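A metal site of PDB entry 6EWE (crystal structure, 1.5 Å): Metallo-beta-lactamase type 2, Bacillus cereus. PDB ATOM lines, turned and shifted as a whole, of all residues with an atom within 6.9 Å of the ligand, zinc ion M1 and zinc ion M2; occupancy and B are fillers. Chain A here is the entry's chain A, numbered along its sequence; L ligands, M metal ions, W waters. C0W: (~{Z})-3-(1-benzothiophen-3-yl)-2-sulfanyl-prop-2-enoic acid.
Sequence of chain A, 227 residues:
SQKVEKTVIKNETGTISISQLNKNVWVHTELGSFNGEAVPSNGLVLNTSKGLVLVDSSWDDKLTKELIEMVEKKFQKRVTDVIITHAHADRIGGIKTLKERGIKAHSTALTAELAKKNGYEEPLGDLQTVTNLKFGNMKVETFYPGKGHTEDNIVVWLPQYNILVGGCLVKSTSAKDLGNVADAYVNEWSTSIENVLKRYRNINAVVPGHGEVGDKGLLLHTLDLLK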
ATOM      1  N   PRO A  40     -20.285   0.091  27.765  1.00  0.00           N
ATOM      2  CA  PRO A  40     -19.521  -0.951  28.458  1.00  0.00           C
ATOM      3  C   PRO A  40     -20.358  -2.190  28.715  1.00  0.00           C
ATOM      4  O   PRO A  40     -21.575  -2.139  28.846  1.00  0.00           O
ATOM      5  CB  PRO A  40     -19.152  -0.282  29.791  1.00  0.00           C
ATOM      6  CG  PRO A  40     -20.330   0.617  30.053  1.00  0.00           C
ATOM      7  CD  PRO A  40     -20.762   1.128  28.702  1.00  0.00           C
ATOM      8  N   SER A  41     -19.645  -3.320  28.745  1.00  0.00           N
ATOM      9  CA  SER A  41     -20.216  -4.629  28.971  1.00  0.00           C
ATOM     10  C   SER A  41     -19.329  -5.376  29.956  1.00  0.00           C
ATOM     11  O   SER A  41     -18.100  -5.260  29.889  1.00  0.00           O
ATOM     12  CB  SER A  41     -20.222  -5.387  27.630  1.00  0.00           C
ATOM     13  OG  SER A  41     -20.570  -6.744  27.791  1.00  0.00           O
ATOM     14  N   TRP A  59     -17.585  -7.712  22.622  1.00  0.00           N
ATOM     15  CA  TRP A  59     -18.422  -7.211  21.534  1.00  0.00           C
ATOM     16  C   TRP A  59     -17.957  -7.723  20.172  1.00  0.00           C
ATOM     17  O   TRP A  59     -18.754  -7.804  19.233  1.00  0.00           O
ATOM     18  CB  TRP A  59     -18.315  -5.692  21.509  1.00  0.00           C
ATOM     19  CG  TRP A  59     -18.898  -5.003  22.715  1.00  0.00           C
ATOM     20  CD1 TRP A  59     -18.228  -4.603  23.844  1.00  0.00           C
ATOM     21  CD2 TRP A  59     -20.267  -4.615  22.899  1.00  0.00           C
ATOM     22  NE1 TRP A  59     -19.107  -3.992  24.718  1.00  0.00           N
ATOM     23  CE2 TRP A  59     -20.358  -3.995  24.168  1.00  0.00           C
ATOM     24  CE3 TRP A  59     -21.423  -4.737  22.113  1.00  0.00           C
ATOM     25  CZ2 TRP A  59     -21.562  -3.483  24.650  1.00  0.00           C
ATOM     26  CZ3 TRP A  59     -22.609  -4.229  22.610  1.00  0.00           C
ATOM     27  CH2 TRP A  59     -22.669  -3.614  23.869  1.00  0.00           C
ATOM     28  N   HIS A  86     -26.066 -15.363  26.543  1.00  0.00           N
ATOM     29  CA  HIS A  86     -27.115 -15.290  25.518  1.00  0.00           C
ATOM     30  C   HIS A  86     -26.452 -14.924  24.184  1.00  0.00           C
ATOM     31  O   HIS A  86     -25.233 -14.755  24.096  1.00  0.00           O
ATOM     32  CB  HIS A  86     -28.242 -14.358  25.950  1.00  0.00           C
ATOM     33  CG  HIS A  86     -27.916 -12.905  25.960  1.00  0.00           C
ATOM     34  ND1 HIS A  86     -27.342 -12.264  27.036  1.00  0.00           N
ATOM     35  CD2 HIS A  86     -28.246 -11.933  25.090  1.00  0.00           C
ATOM     36  CE1 HIS A  86     -27.270 -10.964  26.780  1.00  0.00           C
ATOM     37  NE2 HIS A  86     -27.829 -10.736  25.613  1.00  0.00           N
ATOM     38  N   ALA A  87     -27.235 -14.936  23.113  1.00  0.00           N
ATOM     39  CA  ALA A  87     -26.705 -14.820  21.757  1.00  0.00           C
ATOM     40  C   ALA A  87     -26.680 -13.389  21.179  1.00  0.00           C
ATOM     41  O   ALA A  87     -26.828 -13.219  19.975  1.00  0.00           O
ATOM     42  CB  ALA A  87     -27.466 -15.761  20.829  1.00  0.00           C
ATOM     43  N   HIS A  88     -26.509 -12.337  21.971  1.00  0.00           N
ATOM     44  CA  HIS A  88     -26.240 -11.013  21.423  1.00  0.00           C
ATOM     45  C   HIS A  88     -24.735 -10.743  21.403  1.00  0.00           C
ATOM     46  O   HIS A  88     -23.978 -11.397  22.108  1.00  0.00           O
ATOM     47  CB  HIS A  88     -26.873  -9.949  22.330  1.00  0.00           C
ATOM     48  CG  HIS A  88     -28.366  -9.805  22.215  1.00  0.00           C
ATOM     49  ND1 HIS A  88     -29.155  -9.244  23.225  1.00  0.00           N
ATOM     50  CD2 HIS A  88     -29.219 -10.080  21.200  1.00  0.00           C
ATOM     51  CE1 HIS A  88     -30.417  -9.225  22.831  1.00  0.00           C
ATOM     52  NE2 HIS A  88     -30.476  -9.692  21.594  1.00  0.00           N
ATOM     53  N   ALA A  89     -24.340  -9.701  20.632  1.00  0.00           N
ATOM     54  CA  ALA A  89     -22.929  -9.443  20.303  1.00  0.00           C
ATOM     55  C   ALA A  89     -22.076  -9.171  21.525  1.00  0.00           C
ATOM     56  O   ALA A  89     -20.874  -9.476  21.519  1.00  0.00           O
ATOM     57  CB  ALA A  89     -22.794  -8.242  19.346  1.00  0.00           C
ATOM     58  N   ASP A  90     -22.647  -8.568  22.566  1.00  0.00           N
ATOM     59  CA  ASP A  90     -21.817  -8.289  23.728  1.00  0.00           C
ATOM     60  C   ASP A  90     -21.376  -9.544  24.431  1.00  0.00           C
ATOM     61  O   ASP A  90     -20.350  -9.532  25.107  1.00  0.00           O
ATOM     62  CB  ASP A  90     -22.511  -7.311  24.690  1.00  0.00           C
ATOM     63  CG  ASP A  90     -23.821  -7.804  25.242  1.00  0.00           C
ATOM     64  OD1 ASP A  90     -24.527  -8.567  24.582  1.00  0.00           O
ATOM     65  OD2 ASP A  90     -24.196  -7.382  26.369  1.00  0.00           O
ATOM     66  N   ARG A  91     -22.130 -10.647  24.288  1.00  0.00           N
ATOM     67  CA  ARG A  91     -21.815 -11.907  24.920  1.00  0.00           C
ATOM     68  C   ARG A  91     -21.028 -12.801  23.985  1.00  0.00           C
ATOM     69  O   ARG A  91     -20.119 -13.489  24.427  1.00  0.00           O
ATOM     70  CB  ARG A  91     -23.084 -12.679  25.304  1.00  0.00           C
ATOM     71  CG  ARG A  91     -24.132 -11.849  26.096  1.00  0.00           C
ATOM     72  CD  ARG A  91     -23.659 -11.480  27.509  1.00  0.00           C
ATOM     73  NE  ARG A  91     -23.441 -10.053  27.656  1.00  0.00           N
ATOM     74  CZ  ARG A  91     -22.769  -9.525  28.668  1.00  0.00           C
ATOM     75  NH1 ARG A  91     -22.333 -10.311  29.620  1.00  0.00           N
ATOM     76  NH2 ARG A  91     -22.582  -8.209  28.730  1.00  0.00           N
ATOM     77  N   HIS A 149     -34.716 -10.687  29.293  1.00  0.00           N
ATOM     78  CA  HIS A 149     -34.020  -9.843  28.333  1.00  0.00           C
ATOM     79  C   HIS A 149     -33.997 -10.460  26.943  1.00  0.00           C
ATOM     80  O   HIS A 149     -34.181  -9.778  25.950  1.00  0.00           O
ATOM     81  CB  HIS A 149     -32.570  -9.584  28.855  1.00  0.00           C
ATOM     82  CG  HIS A 149     -31.668  -9.014  27.822  1.00  0.00           C
ATOM     83  ND1 HIS A 149     -31.806  -7.749  27.365  1.00  0.00           N
ATOM     84  CD2 HIS A 149     -30.592  -9.546  27.149  1.00  0.00           C
ATOM     85  CE1 HIS A 149     -30.897  -7.488  26.451  1.00  0.00           C
ATOM     86  NE2 HIS A 149     -30.160  -8.584  26.286  1.00  0.00           N
ATOM     87  N   THR A 150     -33.839 -11.789  26.874  1.00  0.00           N
ATOM     88  CA  THR A 150     -33.970 -12.546  25.662  1.00  0.00           C
ATOM     89  C   THR A 150     -34.578 -13.864  26.047  1.00  0.00           C
ATOM     90  O   THR A 150     -34.788 -14.182  27.217  1.00  0.00           O
ATOM     91  CB  THR A 150     -32.613 -12.904  25.030  1.00  0.00           C
ATOM     92  OG1 THR A 150     -31.819 -13.619  25.979  1.00  0.00           O
ATOM     93  CG2 THR A 150     -31.908 -11.728  24.445  1.00  0.00           C
ATOM     94  N   GLY A 167     -25.905 -11.157  34.107  1.00  0.00           N
ATOM     95  CA  GLY A 167     -25.922 -10.870  32.706  1.00  0.00           C
ATOM     96  C   GLY A 167     -26.961  -9.824  32.433  1.00  0.00           C
ATOM     97  O   GLY A 167     -27.326  -9.017  33.289  1.00  0.00           O
ATOM     98  N   CYS A 168     -27.464  -9.845  31.192  1.00  0.00           N
ATOM     99  CA  CYS A 168     -28.317  -8.777  30.725  1.00  0.00           C
ATOM    100  C   CYS A 168     -29.749  -8.959  31.189  1.00  0.00           C
ATOM    101  O   CYS A 168     -30.514  -8.016  31.062  1.00  0.00           O
ATOM    102  CB  CYS A 168     -28.119  -8.606  29.215  1.00  0.00           C
ATOM    103  SG  CYS A 168     -26.330  -8.448  28.915  1.00  0.00           S
ATOM    104  N   LEU A 169     -30.056 -10.082  31.853  1.00  0.00           N
ATOM    105  CA  LEU A 169     -31.288 -10.233  32.617  1.00  0.00           C
ATOM    106  C   LEU A 169     -31.391  -9.217  33.755  1.00  0.00           C
ATOM    107  O   LEU A 169     -32.503  -8.861  34.170  1.00  0.00           O
ATOM    108  CB  LEU A 169     -31.342 -11.658  33.191  1.00  0.00           C
ATOM    109  CG  LEU A 169     -32.609 -12.038  33.921  1.00  0.00           C
ATOM    110  CD1 LEU A 169     -33.749 -12.266  32.892  1.00  0.00           C
ATOM    111  CD2 LEU A 169     -32.381 -13.279  34.744  1.00  0.00           C
ATOM    112  N   LYS A 171     -30.473  -5.527  35.442  1.00  0.00           N
ATOM    113  CA  LYS A 171     -30.090  -4.149  35.164  1.00  0.00           C
ATOM    114  C   LYS A 171     -29.312  -3.567  36.338  1.00  0.00           C
ATOM    115  O   LYS A 171     -29.581  -3.881  37.495  1.00  0.00           O
ATOM    116  CB  LYS A 171     -31.348  -3.298  34.918  1.00  0.00           C
ATOM    117  CG  LYS A 171     -32.081  -3.674  33.649  1.00  0.00           C
ATOM    118  CD  LYS A 171     -31.240  -3.386  32.430  1.00  0.00           C
ATOM    119  CE  LYS A 171     -31.918  -3.807  31.144  1.00  0.00           C
ATOM    120  NZ  LYS A 171     -31.041  -3.405  29.968  1.00  0.00           N
ATOM    121  N   LEU A 178     -35.397  -0.500  30.569  1.00  0.00           N
ATOM    122  CA  LEU A 178     -34.984  -1.883  30.304  1.00  0.00           C
ATOM    123  C   LEU A 178     -34.034  -2.017  29.125  1.00  0.00           C
ATOM    124  O   LEU A 178     -33.536  -3.134  28.870  1.00  0.00           O
ATOM    125  CB  LEU A 178     -36.236  -2.734  30.068  1.00  0.00           C
ATOM    126  CG  LEU A 178     -37.154  -2.886  31.262  1.00  0.00           C
ATOM    127  CD1 LEU A 178     -38.515  -3.472  30.831  1.00  0.00           C
ATOM    128  CD2 LEU A 178     -36.498  -3.743  32.334  1.00  0.00           C
ATOM    129  N   GLY A 179     -33.767  -0.920  28.406  1.00  0.00           N
ATOM    130  CA  GLY A 179     -32.922  -0.957  27.212  1.00  0.00           C
ATOM    131  C   GLY A 179     -33.690  -1.445  25.993  1.00  0.00           C
ATOM    132  O   GLY A 179     -34.897  -1.291  25.893  1.00  0.00           O
ATOM    133  N   ASN A 180     -32.969  -2.063  25.066  1.00  0.00           N
ATOM    134  CA  ASN A 180     -33.591  -2.589  23.846  1.00  0.00           C
ATOM    135  C   ASN A 180     -34.332  -3.863  24.212  1.00  0.00           C
ATOM    136  O   ASN A 180     -33.726  -4.832  24.670  1.00  0.00           O
ATOM    137  CB  ASN A 180     -32.544  -2.829  22.745  1.00  0.00           C
ATOM    138  CG  ASN A 180     -33.190  -3.158  21.387  1.00  0.00           C
ATOM    139  OD1 ASN A 180     -34.228  -3.781  21.337  1.00  0.00           O
ATOM    140  ND2 ASN A 180     -32.560  -2.727  20.293  1.00  0.00           N
ATOM    141  N   VAL A 181     -35.663  -3.815  24.053  1.00  0.00           N
ATOM    142  CA  VAL A 181     -36.545  -4.920  24.381  1.00  0.00           C
ATOM    143  C   VAL A 181     -37.044  -5.637  23.140  1.00  0.00           C
ATOM    144  O   VAL A 181     -37.973  -6.436  23.231  1.00  0.00           O
ATOM    145  CB  VAL A 181     -37.699  -4.460  25.300  1.00  0.00           C
ATOM    146  CG1 VAL A 181     -37.119  -4.047  26.640  1.00  0.00           C
ATOM    147  CG2 VAL A 181     -38.570  -3.314  24.628  1.00  0.00           C
ATOM    148  N   ALA A 182     -36.412  -5.411  21.975  1.00  0.00           N
ATOM    149  CA  ALA A 182     -36.879  -6.056  20.746  1.00  0.00           C
ATOM    150  C   ALA A 182     -36.874  -7.577  20.875  1.00  0.00           C
ATOM    151  O   ALA A 182     -37.771  -8.249  20.334  1.00  0.00           O
ATOM    152  CB  ALA A 182     -36.026  -5.634  19.540  1.00  0.00           C
ATOM    153  N   ASP A 183     -35.888  -8.140  21.579  1.00  0.00           N
ATOM    154  CA  ASP A 183     -35.782  -9.579  21.750  1.00  0.00           C
ATOM    155  C   ASP A 183     -36.299 -10.041  23.096  1.00  0.00           C
ATOM    156  O   ASP A 183     -36.091 -11.185  23.465  1.00  0.00           O
ATOM    157  CB  ASP A 183     -34.317 -10.063  21.566  1.00  0.00           C
ATOM    158  CG  ASP A 183     -33.811  -9.889  20.145  1.00  0.00           C
ATOM    159  OD1 ASP A 183     -34.638  -9.721  19.211  1.00  0.00           O
ATOM    160  OD2 ASP A 183     -32.573  -9.969  19.958  1.00  0.00           O
ATOM    161  N   ALA A 184     -36.988  -9.162  23.850  1.00  0.00           N
ATOM    162  CA  ALA A 184     -37.298  -9.395  25.247  1.00  0.00           C
ATOM    163  C   ALA A 184     -38.735  -9.885  25.437  1.00  0.00           C
ATOM    164  O   ALA A 184     -39.578  -9.802  24.527  1.00  0.00           O
ATOM    165  CB  ALA A 184     -37.087  -8.106  26.050  1.00  0.00           C
ATOM    166  N   GLY A 209     -25.052  -7.292  33.346  1.00  0.00           N
ATOM    167  CA  GLY A 209     -24.396  -7.307  32.034  1.00  0.00           C
ATOM    168  C   GLY A 209     -23.730  -5.992  31.676  1.00  0.00           C
ATOM    169  O   GLY A 209     -22.727  -5.971  30.949  1.00  0.00           O
ATOM    170  N   HIS A 210     -24.247  -4.899  32.184  1.00  0.00           N
ATOM    171  CA  HIS A 210     -23.741  -3.550  31.953  1.00  0.00           C
ATOM    172  C   HIS A 210     -23.880  -2.774  33.258  1.00  0.00           C
ATOM    173  O   HIS A 210     -24.932  -2.827  33.908  1.00  0.00           O
ATOM    174  CB  HIS A 210     -24.509  -2.864  30.800  1.00  0.00           C
ATOM    175  CG  HIS A 210     -24.658  -3.733  29.569  1.00  0.00           C
ATOM    176  ND1 HIS A 210     -23.774  -3.698  28.524  1.00  0.00           N
ATOM    177  CD2 HIS A 210     -25.622  -4.634  29.226  1.00  0.00           C
ATOM    178  CE1 HIS A 210     -24.147  -4.574  27.596  1.00  0.00           C
ATOM    179  NE2 HIS A 210     -25.280  -5.138  27.986  1.00  0.00           N
HETATM  180  C4  C0W L   1     -27.695  -5.920  22.098  1.00  0.00           C
HETATM  181  C5  C0W L   1     -29.645  -6.380  20.621  1.00  0.00           C
HETATM  182  C6  C0W L   1     -30.587  -6.722  19.658  1.00  0.00           C
HETATM  183  C7  C0W L   1     -31.921  -6.706  19.989  1.00  0.00           C
HETATM  184  C8  C0W L   1     -32.322  -6.344  21.268  1.00  0.00           C
HETATM  185  C9  C0W L   1     -31.384  -5.971  22.217  1.00  0.00           C
HETATM  186  C10 C0W L   1     -30.021  -5.980  21.918  1.00  0.00           C
HETATM  187  C   C0W L   1     -28.585  -5.281  26.635  1.00  0.00           C
HETATM  188  O   C0W L   1     -29.404  -4.232  26.726  1.00  0.00           O
HETATM  189  C1  C0W L   1     -28.307  -5.761  25.268  1.00  0.00           C
HETATM  190  C2  C0W L   1     -28.981  -5.330  24.166  1.00  0.00           C
HETATM  191  C3  C0W L   1     -28.878  -5.715  22.764  1.00  0.00           C
HETATM  192  O1  C0W L   1     -28.133  -5.847  27.588  1.00  0.00           O
HETATM  193  S   C0W L   1     -27.081  -7.032  25.113  1.00  0.00           S
HETATM  194  S1  C0W L   1     -27.907  -6.436  20.466  1.00  0.00           S
HETATM  195 ZN    ZN M   1     -28.482  -8.874  25.100  1.00  0.00          ZN
HETATM  196 ZN    ZN M   2     -26.146  -6.865  27.186  1.00  0.00          ZN
HETATM  197  O   HOH W   1     -30.178  -2.231  25.401  1.00  0.00           O
HETATM  198  O   HOH W   2     -29.199  -5.622  30.209  1.00  0.00           O
HETATM  199  O   HOH W   3     -33.859  -7.645  23.968  1.00  0.00           O
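The side-chain amino group (NZ) of Lys 171 lies within salt-bridge range of an oxygen (O) of the ligand.
Zinc ion M1 is bound by a ring nitrogen (ND1) of His 88 (2.0 Å), a ring nitrogen (NE2) of His 86 (2.0 Å), a ring nitrogen (NE2) of His 149 (2.1 Å) and a sulfur (S) of the ligand (2.3 Å). Zinc ion M1 has four donor atoms within binding distance.
Zinc ion M2 is bound by a ring nitrogen (NE2) of His 210 (2.1 Å), the side-chain carboxylate of Asp 90 (2.2 Å), an oxygen (O1) of the ligand (2.3 Å), a sulfur (S) of the ligand (2.3 Å) and the side-chain sulfur of Cys 168 (2.4 Å).
The nearest printed residue that does not touch zinc ion M1 is Asp 90 (4.001 Å).
Water W1 lies within hydrogen-bond range of an oxygen (O) of the ligand (2.5 Å) and the backbone NH (N) of Asn 180 (2.8 Å). Water W2 lies within hydrogen-bond range of the backbone carbonyl oxygen of Cys 168 (2.9 Å) and the side-chain amino group of Lys 171 (2.9 Å). Water W3 lies within hydrogen-bond range of the backbone carbonyl oxygen (O) of Asn 180 (2.9 Å), the backbone carbonyl oxygen (O) of His 149 (2.9 Å), the backbone NH (N) of Asp 183 (3.2 Å) and the backbone NH (N) of Ala 184 (3.5 Å).
The side-chain carboxylate of Asp 90 is in salt-bridge range of the guanidinium group of Arg 91, at 3.6 Å. N of Ala 182 lies within hydrogen-bond range of OD1 of Asn 180. O of Leu 178 is in hydrogen-bond range of NZ of Lys 171 (2.7 Å). OD2 of Asp 183 lies within hydrogen-bond range of NE2 of His 88. The guanidinium group (NE) of Arg 91 sits close to the side-chain sulfur (SG) of Cys 168 (3.5 Å). The backbone carbonyl oxygen (O) of Pro 40 lies within hydrogen-bond range of a ring nitrogen (ND1) of His 210, 2.7 Å away.
Asn 180 touches the ligand. OD2 of Asp 183 touches C7 of the ligand, at 3.3 Å. Of the 24 residues printed, 9 come within 4 Å of the ligand.
Within 4 Å of zinc ion M2: Asp 90, Cys 168 and His 210. Along chain A the residues within 4 Å of zinc ion M2 span positions 90 to 210.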
